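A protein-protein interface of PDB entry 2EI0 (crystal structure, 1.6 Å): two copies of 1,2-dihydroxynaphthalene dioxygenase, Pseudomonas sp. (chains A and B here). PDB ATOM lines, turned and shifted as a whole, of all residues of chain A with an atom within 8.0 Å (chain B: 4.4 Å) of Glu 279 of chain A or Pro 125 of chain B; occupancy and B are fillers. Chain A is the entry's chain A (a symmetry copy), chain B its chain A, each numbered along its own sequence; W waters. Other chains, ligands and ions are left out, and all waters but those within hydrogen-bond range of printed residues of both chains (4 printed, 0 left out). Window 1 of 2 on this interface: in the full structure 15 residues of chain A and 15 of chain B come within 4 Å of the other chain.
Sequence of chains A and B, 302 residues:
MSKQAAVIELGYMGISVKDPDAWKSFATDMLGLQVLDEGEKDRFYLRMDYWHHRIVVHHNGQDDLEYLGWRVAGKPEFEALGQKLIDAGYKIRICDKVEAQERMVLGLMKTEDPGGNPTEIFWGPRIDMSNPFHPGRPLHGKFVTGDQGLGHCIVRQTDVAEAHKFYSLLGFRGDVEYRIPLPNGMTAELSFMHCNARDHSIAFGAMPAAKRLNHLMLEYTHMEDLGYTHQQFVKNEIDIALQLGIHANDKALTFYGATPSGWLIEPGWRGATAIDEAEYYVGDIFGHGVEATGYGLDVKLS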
ATOM      1  N   ASP A 175      25.316  16.936   9.733  1.00  0.00           N
ATOM      2  CA  ASP A 175      26.590  16.240   9.607  1.00  0.00           C
ATOM      3  C   ASP A 175      26.313  14.808   9.175  1.00  0.00           C
ATOM      4  O   ASP A 175      25.247  14.534   8.609  1.00  0.00           O
ATOM      5  CB  ASP A 175      27.363  16.314  10.930  1.00  0.00           C
ATOM      6  CG  ASP A 175      28.865  16.399  10.718  1.00  0.00           C
ATOM      7  OD1 ASP A 175      29.446  15.396  10.262  1.00  0.00           O
ATOM      8  OD2 ASP A 175      29.462  17.468  10.999  1.00  0.00           O
ATOM      9  N   VAL A 176      27.260  13.908   9.423  1.00  0.00           N
ATOM     10  CA  VAL A 176      27.092  12.488   9.114  1.00  0.00           C
ATOM     11  C   VAL A 176      25.910  11.917   9.898  1.00  0.00           C
ATOM     12  O   VAL A 176      25.906  11.959  11.132  1.00  0.00           O
ATOM     13  CB  VAL A 176      28.374  11.704   9.466  1.00  0.00           C
ATOM     14  CG1 VAL A 176      28.140  10.192   9.381  1.00  0.00           C
ATOM     15  CG2 VAL A 176      29.513  12.140   8.560  1.00  0.00           C
ATOM     16  N   GLU A 177      24.908  11.397   9.182  1.00  0.00           N
ATOM     17  CA  GLU A 177      23.761  10.765   9.840  1.00  0.00           C
ATOM     18  C   GLU A 177      23.657   9.266   9.600  1.00  0.00           C
ATOM     19  O   GLU A 177      22.921   8.573  10.294  1.00  0.00           O
ATOM     20  CB  GLU A 177      22.449  11.471   9.463  1.00  0.00           C
ATOM     21  CG  GLU A 177      22.349  12.865  10.064  1.00  0.00           C
ATOM     22  CD  GLU A 177      21.086  13.605   9.668  1.00  0.00           C
ATOM     23  OE1 GLU A 177      20.285  13.080   8.873  1.00  0.00           O
ATOM     24  OE2 GLU A 177      20.895  14.728  10.164  1.00  0.00           O
ATOM     25  N   TYR A 178      24.390   8.746   8.620  1.00  0.00           N
ATOM     26  CA  TYR A 178      24.424   7.300   8.458  1.00  0.00           C
ATOM     27  C   TYR A 178      25.831   6.809   8.320  1.00  0.00           C
ATOM     28  O   TYR A 178      26.634   7.424   7.621  1.00  0.00           O
ATOM     29  CB  TYR A 178      23.651   6.846   7.222  1.00  0.00           C
ATOM     30  CG  TYR A 178      22.148   6.963   7.349  1.00  0.00           C
ATOM     31  CD1 TYR A 178      21.515   8.171   7.096  1.00  0.00           C
ATOM     32  CD2 TYR A 178      21.363   5.868   7.715  1.00  0.00           C
ATOM     33  CE1 TYR A 178      20.134   8.309   7.184  1.00  0.00           C
ATOM     34  CE2 TYR A 178      19.953   6.002   7.814  1.00  0.00           C
ATOM     35  CZ  TYR A 178      19.367   7.220   7.537  1.00  0.00           C
ATOM     36  OH  TYR A 178      17.989   7.393   7.609  1.00  0.00           O
ATOM     37  N   ARG A 179      26.109   5.691   8.987  1.00  0.00           N
ATOM     38  CA  ARG A 179      27.374   4.981   8.817  1.00  0.00           C
ATOM     39  C   ARG A 179      26.989   3.582   8.354  1.00  0.00           C
ATOM     40  O   ARG A 179      26.492   2.784   9.148  1.00  0.00           O
ATOM     41  CB  ARG A 179      28.177   4.954  10.128  1.00  0.00           C
ATOM     42  CG  ARG A 179      28.597   6.350  10.621  1.00  0.00           C
ATOM     43  CD  ARG A 179      29.700   6.321  11.692  1.00  0.00           C
ATOM     44  NE  ARG A 179      31.020   6.190  11.075  1.00  0.00           N
ATOM     45  CZ  ARG A 179      31.773   5.093  11.107  1.00  0.00           C
ATOM     46  NH1 ARG A 179      31.370   4.007  11.759  1.00  0.00           N
ATOM     47  NH2 ARG A 179      32.949   5.083  10.497  1.00  0.00           N
ATOM     48  N   LEU A 190      27.297   9.161   5.231  1.00  0.00           N
ATOM     49  CA  LEU A 190      26.412  10.030   4.447  1.00  0.00           C
ATOM     50  C   LEU A 190      26.004  11.210   5.305  1.00  0.00           C
ATOM     51  O   LEU A 190      25.545  11.016   6.429  1.00  0.00           O
ATOM     52  CB  LEU A 190      25.160   9.267   4.000  1.00  0.00           C
ATOM     53  CG  LEU A 190      25.399   7.876   3.393  1.00  0.00           C
ATOM     54  CD1 LEU A 190      24.072   7.217   3.073  1.00  0.00           C
ATOM     55  CD2 LEU A 190      26.263   7.939   2.154  1.00  0.00           C
ATOM     56  N   PHE A 192      23.846  14.908   5.889  1.00  0.00           N
ATOM     57  CA  PHE A 192      22.533  15.470   5.545  1.00  0.00           C
ATOM     58  C   PHE A 192      22.405  16.820   6.215  1.00  0.00           C
ATOM     59  O   PHE A 192      22.635  16.926   7.424  1.00  0.00           O
ATOM     60  CB  PHE A 192      21.403  14.567   6.051  1.00  0.00           C
ATOM     61  CG  PHE A 192      21.378  13.196   5.427  1.00  0.00           C
ATOM     62  CD1 PHE A 192      22.258  12.198   5.868  1.00  0.00           C
ATOM     63  CD2 PHE A 192      20.440  12.877   4.441  1.00  0.00           C
ATOM     64  CE1 PHE A 192      22.232  10.925   5.303  1.00  0.00           C
ATOM     65  CE2 PHE A 192      20.425  11.601   3.870  1.00  0.00           C
ATOM     66  CZ  PHE A 192      21.310  10.631   4.312  1.00  0.00           C
ATOM     67  N   ASP A 199      13.510  17.996   6.945  1.00  0.00           N
ATOM     68  CA  ASP A 199      14.574  17.285   7.654  1.00  0.00           C
ATOM     69  C   ASP A 199      15.940  17.449   6.979  1.00  0.00           C
ATOM     70  O   ASP A 199      16.948  17.655   7.645  1.00  0.00           O
ATOM     71  CB  ASP A 199      14.263  15.808   7.812  1.00  0.00           C
ATOM     72  CG  ASP A 199      15.411  15.071   8.470  1.00  0.00           C
ATOM     73  OD1 ASP A 199      15.477  15.103   9.718  1.00  0.00           O
ATOM     74  OD2 ASP A 199      16.256  14.543   7.729  1.00  0.00           O
ATOM     75  N   ALA A 248      15.402   6.455   8.667  1.00  0.00           N
ATOM     76  CA  ALA A 248      15.626   6.682  10.098  1.00  0.00           C
ATOM     77  C   ALA A 248      15.729   8.172  10.437  1.00  0.00           C
ATOM     78  O   ALA A 248      15.267   8.596  11.497  1.00  0.00           O
ATOM     79  CB  ALA A 248      16.856   5.920  10.587  1.00  0.00           C
ATOM     80  N   ASN A 249      16.308   8.966   9.536  1.00  0.00           N
ATOM     81  CA  ASN A 249      16.423  10.401   9.804  1.00  0.00           C
ATOM     82  C   ASN A 249      15.121  11.207   9.660  1.00  0.00           C
ATOM     83  O   ASN A 249      14.655  11.776  10.640  1.00  0.00           O
ATOM     84  CB  ASN A 249      17.629  11.070   9.095  1.00  0.00           C
ATOM     85  CG  ASN A 249      17.600  10.954   7.580  1.00  0.00           C
ATOM     86  OD1 ASN A 249      16.638  10.472   6.978  1.00  0.00           O
ATOM     87  ND2 ASN A 249      18.680  11.427   6.948  1.00  0.00           N
ATOM     88  N   LYS A 251      12.038  10.085   8.741  1.00  0.00           N
ATOM     89  CA  LYS A 251      10.838   9.311   9.072  1.00  0.00           C
ATOM     90  C   LYS A 251       9.799   9.303   7.934  1.00  0.00           C
ATOM     91  O   LYS A 251       8.645   8.951   8.169  1.00  0.00           O
ATOM     92  CB  LYS A 251      10.140   9.811  10.365  1.00  0.00           C
ATOM     93  CG  LYS A 251      11.018  10.153  11.594  1.00  0.00           C
ATOM     94  CD  LYS A 251      11.966   9.036  11.970  1.00  0.00           C
ATOM     95  CE  LYS A 251      12.668   9.360  13.292  1.00  0.00           C
ATOM     96  NZ  LYS A 251      13.751  10.390  13.135  1.00  0.00           N
ATOM     97  N   ILE A 275      16.025  18.430  13.016  1.00  0.00           N
ATOM     98  CA  ILE A 275      16.533  18.690  14.371  1.00  0.00           C
ATOM     99  C   ILE A 275      17.981  19.112  14.350  1.00  0.00           C
ATOM    100  O   ILE A 275      18.753  18.611  13.534  1.00  0.00           O
ATOM    101  CB  ILE A 275      16.342  17.492  15.317  1.00  0.00           C
ATOM    102  CG1 ILE A 275      17.083  16.252  14.805  1.00  0.00           C
ATOM    103  CG2 ILE A 275      14.848  17.212  15.549  1.00  0.00           C
ATOM    104  CD1 ILE A 275      17.116  15.130  15.825  1.00  0.00           C
ATOM    105  N   ASP A 276      18.349  20.030  15.254  1.00  0.00           N
ATOM    106  CA  ASP A 276      19.730  20.505  15.336  1.00  0.00           C
ATOM    107  C   ASP A 276      20.611  19.577  16.158  1.00  0.00           C
ATOM    108  O   ASP A 276      21.841  19.720  16.132  1.00  0.00           O
ATOM    109  CB  ASP A 276      19.806  21.923  15.935  1.00  0.00           C
ATOM    110  CG  ASP A 276      19.536  23.030  14.917  1.00  0.00           C
ATOM    111  OD1 ASP A 276      19.244  22.745  13.739  1.00  0.00           O
ATOM    112  OD2 ASP A 276      19.613  24.211  15.320  1.00  0.00           O
ATOM    113  N   GLU A 277      20.001  18.635  16.887  1.00  0.00           N
ATOM    114  CA  GLU A 277      20.778  17.668  17.664  1.00  0.00           C
ATOM    115  C   GLU A 277      21.198  16.508  16.771  1.00  0.00           C
ATOM    116  O   GLU A 277      20.375  15.701  16.362  1.00  0.00           O
ATOM    117  CB  GLU A 277      19.990  17.178  18.882  1.00  0.00           C
ATOM    118  CG  GLU A 277      19.553  18.291  19.832  1.00  0.00           C
ATOM    119  CD  GLU A 277      18.361  19.099  19.321  1.00  0.00           C
ATOM    120  OE1 GLU A 277      17.509  18.532  18.595  1.00  0.00           O
ATOM    121  OE2 GLU A 277      18.299  20.310  19.627  1.00  0.00           O
ATOM    122  N   ALA A 278      22.495  16.449  16.476  1.00  0.00           N
ATOM    123  CA  ALA A 278      23.054  15.433  15.594  1.00  0.00           C
ATOM    124  C   ALA A 278      22.873  14.011  16.150  1.00  0.00           C
ATOM    125  O   ALA A 278      23.224  13.744  17.303  1.00  0.00           O
ATOM    126  CB  ALA A 278      24.545  15.735  15.346  1.00  0.00           C
ATOM    127  N   GLU A 279      22.322  13.120  15.317  1.00  0.00           N
ATOM    128  CA  GLU A 279      22.147  11.677  15.606  1.00  0.00           C
ATOM    129  C   GLU A 279      22.749  10.922  14.434  1.00  0.00           C
ATOM    130  O   GLU A 279      22.815  11.467  13.318  1.00  0.00           O
ATOM    131  CB  GLU A 279      20.640  11.306  15.638  1.00  0.00           C
ATOM    132  CG  GLU A 279      19.824  11.898  16.775  1.00  0.00           C
ATOM    133  CD  GLU A 279      18.354  11.500  16.741  1.00  0.00           C
ATOM    134  OE1 GLU A 279      17.634  11.886  17.688  1.00  0.00           O
ATOM    135  OE2 GLU A 279      17.884  10.812  15.795  1.00  0.00           O
ATOM    136  N   TYR A 280      23.170   9.672  14.637  1.00  0.00           N
ATOM    137  CA  TYR A 280      23.403   8.817  13.461  1.00  0.00           C
ATOM    138  C   TYR A 280      22.787   7.429  13.593  1.00  0.00           C
ATOM    139  O   TYR A 280      22.463   6.977  14.696  1.00  0.00           O
ATOM    140  CB  TYR A 280      24.889   8.705  13.083  1.00  0.00           C
ATOM    141  CG  TYR A 280      25.701   7.726  13.901  1.00  0.00           C
ATOM    142  CD1 TYR A 280      26.227   8.091  15.144  1.00  0.00           C
ATOM    143  CD2 TYR A 280      25.973   6.449  13.419  1.00  0.00           C
ATOM    144  CE1 TYR A 280      26.991   7.200  15.893  1.00  0.00           C
ATOM    145  CE2 TYR A 280      26.745   5.545  14.156  1.00  0.00           C
ATOM    146  CZ  TYR A 280      27.249   5.927  15.394  1.00  0.00           C
ATOM    147  OH  TYR A 280      28.020   5.048  16.132  1.00  0.00           O
ATOM    148  N   TYR A 281      22.641   6.771  12.440  1.00  0.00           N
ATOM    149  CA  TYR A 281      22.011   5.466  12.335  1.00  0.00           C
ATOM    150  C   TYR A 281      22.873   4.562  11.481  1.00  0.00           C
ATOM    151  O   TYR A 281      23.743   5.031  10.735  1.00  0.00           O
ATOM    152  CB  TYR A 281      20.632   5.605  11.673  1.00  0.00           C
ATOM    153  CG  TYR A 281      19.926   6.885  12.071  1.00  0.00           C
ATOM    154  CD1 TYR A 281      19.171   6.947  13.237  1.00  0.00           C
ATOM    155  CD2 TYR A 281      20.033   8.039  11.289  1.00  0.00           C
ATOM    156  CE1 TYR A 281      18.542   8.126  13.631  1.00  0.00           C
ATOM    157  CE2 TYR A 281      19.405   9.221  11.665  1.00  0.00           C
ATOM    158  CZ  TYR A 281      18.664   9.259  12.839  1.00  0.00           C
ATOM    159  OH  TYR A 281      18.038  10.429  13.219  1.00  0.00           O
ATOM    160  N   TRP B  51      17.800   4.752  21.465  1.00  0.00           N
ATOM    161  CA  TRP B  51      19.274   4.785  21.471  1.00  0.00           C
ATOM    162  C   TRP B  51      19.814   3.368  21.455  1.00  0.00           C
ATOM    163  O   TRP B  51      19.220   2.462  22.048  1.00  0.00           O
ATOM    164  CB  TRP B  51      19.790   5.534  22.696  1.00  0.00           C
ATOM    165  CG  TRP B  51      19.639   7.035  22.585  1.00  0.00           C
ATOM    166  CD1 TRP B  51      18.564   7.739  22.093  1.00  0.00           C
ATOM    167  CD2 TRP B  51      20.593   8.012  23.020  1.00  0.00           C
ATOM    168  NE1 TRP B  51      18.811   9.096  22.182  1.00  0.00           N
ATOM    169  CE2 TRP B  51      20.049   9.286  22.747  1.00  0.00           C
ATOM    170  CE3 TRP B  51      21.867   7.926  23.606  1.00  0.00           C
ATOM    171  CZ2 TRP B  51      20.740  10.472  23.039  1.00  0.00           C
ATOM    172  CZ3 TRP B  51      22.544   9.093  23.914  1.00  0.00           C
ATOM    173  CH2 TRP B  51      21.979  10.358  23.621  1.00  0.00           C
ATOM    174  N   ARG B  71      25.979  14.980  26.386  1.00  0.00           N
ATOM    175  CA  ARG B  71      25.789  15.261  24.964  1.00  0.00           C
ATOM    176  C   ARG B  71      25.769  16.757  24.702  1.00  0.00           C
ATOM    177  O   ARG B  71      25.185  17.518  25.491  1.00  0.00           O
ATOM    178  CB  ARG B  71      24.454  14.673  24.507  1.00  0.00           C
ATOM    179  CG  ARG B  71      24.211  14.723  23.003  1.00  0.00           C
ATOM    180  CD  ARG B  71      22.776  14.308  22.720  1.00  0.00           C
ATOM    181  NE  ARG B  71      22.538  14.248  21.279  1.00  0.00           N
ATOM    182  CZ  ARG B  71      21.347  14.029  20.722  1.00  0.00           C
ATOM    183  NH1 ARG B  71      20.262  13.836  21.474  1.00  0.00           N
ATOM    184  NH2 ARG B  71      21.249  13.986  19.401  1.00  0.00           N
ATOM    185  N   MET B 104      30.334   4.537  20.559  1.00  0.00           N
ATOM    186  CA  MET B 104      29.327   4.679  19.485  1.00  0.00           C
ATOM    187  C   MET B 104      28.828   6.113  19.338  1.00  0.00           C
ATOM    188  O   MET B 104      27.617   6.376  19.302  1.00  0.00           O
ATOM    189  CB  MET B 104      28.173   3.688  19.652  1.00  0.00           C
ATOM    190  CG  MET B 104      28.670   2.236  19.599  1.00  0.00           C
ATOM    191  SD  MET B 104      27.372   1.060  19.994  1.00  0.00           S
ATOM    192  CE  MET B 104      28.343  -0.367  20.451  1.00  0.00           C
ATOM    193  N   PHE B 122      30.335  14.476  24.288  1.00  0.00           N
ATOM    194  CA  PHE B 122      30.232  13.871  22.965  1.00  0.00           C
ATOM    195  C   PHE B 122      29.163  14.535  22.136  1.00  0.00           C
ATOM    196  O   PHE B 122      28.302  15.249  22.659  1.00  0.00           O
ATOM    197  CB  PHE B 122      29.934  12.366  23.075  1.00  0.00           C
ATOM    198  CG  PHE B 122      28.509  12.045  23.457  1.00  0.00           C
ATOM    199  CD1 PHE B 122      28.101  12.059  24.800  1.00  0.00           C
ATOM    200  CD2 PHE B 122      27.583  11.728  22.474  1.00  0.00           C
ATOM    201  CE1 PHE B 122      26.779  11.755  25.152  1.00  0.00           C
ATOM    202  CE2 PHE B 122      26.252  11.426  22.806  1.00  0.00           C
ATOM    203  CZ  PHE B 122      25.853  11.440  24.149  1.00  0.00           C
ATOM    204  N   TRP B 123      29.219  14.280  20.834  1.00  0.00           N
ATOM    205  CA  TRP B 123      28.100  14.587  19.966  1.00  0.00           C
ATOM    206  C   TRP B 123      27.854  13.401  19.050  1.00  0.00           C
ATOM    207  O   TRP B 123      28.761  12.614  18.788  1.00  0.00           O
ATOM    208  CB  TRP B 123      28.331  15.873  19.148  1.00  0.00           C
ATOM    209  CG  TRP B 123      29.412  15.748  18.092  1.00  0.00           C
ATOM    210  CD1 TRP B 123      30.774  15.874  18.270  1.00  0.00           C
ATOM    211  CD2 TRP B 123      29.218  15.463  16.706  1.00  0.00           C
ATOM    212  NE1 TRP B 123      31.423  15.692  17.077  1.00  0.00           N
ATOM    213  CE2 TRP B 123      30.496  15.436  16.101  1.00  0.00           C
ATOM    214  CE3 TRP B 123      28.086  15.231  15.915  1.00  0.00           C
ATOM    215  CZ2 TRP B 123      30.677  15.185  14.738  1.00  0.00           C
ATOM    216  CZ3 TRP B 123      28.262  14.989  14.545  1.00  0.00           C
ATOM    217  CH2 TRP B 123      29.552  14.964  13.978  1.00  0.00           C
ATOM    218  N   GLY B 124      26.618  13.286  18.581  1.00  0.00           N
ATOM    219  CA  GLY B 124      26.258  12.258  17.607  1.00  0.00           C
ATOM    220  C   GLY B 124      26.130  10.855  18.170  1.00  0.00           C
ATOM    221  O   GLY B 124      26.889   9.961  17.800  1.00  0.00           O
ATOM    222  N   PRO B 125      25.127  10.633  19.033  1.00  0.00           N
ATOM    223  CA  PRO B 125      24.887   9.278  19.518  1.00  0.00           C
ATOM    224  C   PRO B 125      24.329   8.397  18.401  1.00  0.00           C
ATOM    225  O   PRO B 125      23.736   8.909  17.440  1.00  0.00           O
ATOM    226  CB  PRO B 125      23.793   9.485  20.570  1.00  0.00           C
ATOM    227  CG  PRO B 125      23.037  10.689  20.073  1.00  0.00           C
ATOM    228  CD  PRO B 125      24.138  11.593  19.572  1.00  0.00           C
ATOM    229  N   ARG B 126      24.530   7.092  18.546  1.00  0.00           N
ATOM    230  CA  ARG B 126      23.944   6.103  17.653  1.00  0.00           C
ATOM    231  C   ARG B 126      22.529   5.788  18.098  1.00  0.00           C
ATOM    232  O   ARG B 126      22.293   5.372  19.243  1.00  0.00           O
ATOM    233  CB  ARG B 126      24.768   4.812  17.653  1.00  0.00           C
ATOM    234  CG  ARG B 126      24.125   3.724  16.789  1.00  0.00           C
ATOM    235  CD  ARG B 126      24.937   2.446  16.776  1.00  0.00           C
ATOM    236  NE  ARG B 126      24.112   1.287  16.420  1.00  0.00           N
ATOM    237  CZ  ARG B 126      24.600   0.078  16.158  1.00  0.00           C
ATOM    238  NH1 ARG B 126      25.912  -0.123  16.179  1.00  0.00           N
ATOM    239  NH2 ARG B 126      23.787  -0.924  15.860  1.00  0.00           N
ATOM    240  N   ILE B 127      21.590   5.988  17.184  1.00  0.00           N
ATOM    241  CA  ILE B 127      20.183   5.712  17.432  1.00  0.00           C
ATOM    242  C   ILE B 127      19.755   4.533  16.570  1.00  0.00           C
ATOM    243  O   ILE B 127      19.945   4.546  15.343  1.00  0.00           O
ATOM    244  CB  ILE B 127      19.299   6.922  17.067  1.00  0.00           C
ATOM    245  CG1 ILE B 127      19.856   8.226  17.656  1.00  0.00           C
ATOM    246  CG2 ILE B 127      17.818   6.674  17.460  1.00  0.00           C
ATOM    247  CD1 ILE B 127      20.169   8.194  19.115  1.00  0.00           C
HETATM  248  O   HOH W   1      24.586  15.134  19.484  1.00  0.00           O
HETATM  249  O   HOH W   2      18.317  13.835  19.248  1.00  0.00           O
HETATM  250  O   HOH W   3      28.362   2.111  15.553  1.00  0.00           O
HETATM  251  O   HOH W   4      17.186  11.040  20.392  1.00  0.00           O
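Asp 199 of chain A touches none of the printed residues of chain B.
Ala 248 of chain A touches none of the printed residues of chain B.
Of the printed residues of chain B, Glu 277 of chain A touches Arg 71.
Printed residues of chain B within 4 Å of Glu 279 of chain A: Arg 71 (3.6 Å), Pro 125 (3.7 Å) and Ile 127 (3.7 Å).
Gly 124 of chain B touches just these residues of chain A: Ala 278 (3.4 Å) and Tyr 280 (3.3 Å).
Pro 125 of chain B touches just these residues of chain A: Ala 278, Glu 279 and Tyr 280.
Printed residues of chain A within 4 Å of Arg 126 of chain B: Tyr 280 (3.4 Å).
The nearest printed residue of chain A that does not touch Met 104 of chain B is Arg 179 of chain A (7.7 Å).
The backbone NH (N) of Tyr 280 of chain A sits at hydrogen-bond distance from the backbone carbonyl oxygen (O) of Pro 125 of chain B (3.0 Å).
The backbone NH (N) of Ile 127 of chain B is in hydrogen-bond range of the backbone carbonyl oxygen (O) of Tyr 280 of chain A (2.8 Å).
The guanidinium group (NH2) of Arg 71 of chain B lies within hydrogen-bond range of the backbone carbonyl oxygen (O) of Ala 278 of chain A.
The backbone carbonyl oxygen (O) of Met 104 of chain B lies within hydrogen-bond range of the side-chain hydroxyl (OH) of Tyr 280 of chain A (3.5 Å).
O of Tyr 281 of chain A is in hydrogen-bond range of N of Arg 179 of chain A.
The backbone carbonyl oxygen of Met 104 of chain B lies within hydrogen-bond range of the backbone NH of Arg 126 of chain B.
The backbone carbonyl oxygen (O) of Asp 175 of chain A sits at hydrogen-bond distance from the backbone NH (N) of Phe 192 of chain A (3.1 Å).
OH of Tyr 281 of chain A sits at hydrogen-bond distance from OE2 of Glu 279 of chain A, 2.6 Å away.
O of Glu 177 of chain A sits at hydrogen-bond distance from N of Tyr 281 of chain A, 2.8 Å away.
Water W2 lies within hydrogen-bond range of the side-chain carboxylate of Glu 279 of chain A (2.6 Å) and the guanidinium group of Arg 71 of chain B (2.9 Å).
Water W1 lies within hydrogen-bond range of the guanidinium group of Arg 71 of chain B, the backbone NH of Gly 124 of chain B and the backbone carbonyl oxygen of Ala 278 of chain A.
Water W4 lies within hydrogen-bond range of OE1 of Glu 279 of chain A (2.9 Å) and NE1 of Trp 51 of chain B (3.1 Å).
Water W3 lies within hydrogen-bond range of the side-chain hydroxyl of Tyr 280 of chain A and the guanidinium group of Arg 126 of chain B.
No position is printed for both chains.
Hydrophobic or aromatic side chains of chain B within 4 Å of the printed part of chain A: Met 104, Trp 123, Pro 125 and Ile 127.
Of the 18 printed residues of chain A, 6 touch a printed residue of chain B.
Along chain A the printed residues that touch a printed residue of chain B span positions 175 to 281.
Among the printed residues, 15 pairs touch across the chains.
Among the printed residues, no Asp or Glu carboxylate lies within 4 Å of a Lys or Arg side-chain nitrogen of the other chain.
Among the printed residues, merely in contact across the chains: Ala 278 of chain A with Pro 125 of chain B, Tyr 281 of chain A with Ile 127 of chain B, Tyr 280 of chain A with Gly 124 of chain B, Ala 278 of chain A with Gly 124 of chain B, Tyr 280 of chain A with Arg 126 of chain B, Glu 277 of chain A with Arg 71 of chain B, Ala 278 of chain A with Trp 123 of chain B, Asp 175 of chain A with Trp 123 of chain B, Glu 279 of chain A with Arg 71 of chain B, Glu 279 of chain A with Pro 125 of chain B and Glu 279 of chain A with Ile 127 of chain B.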
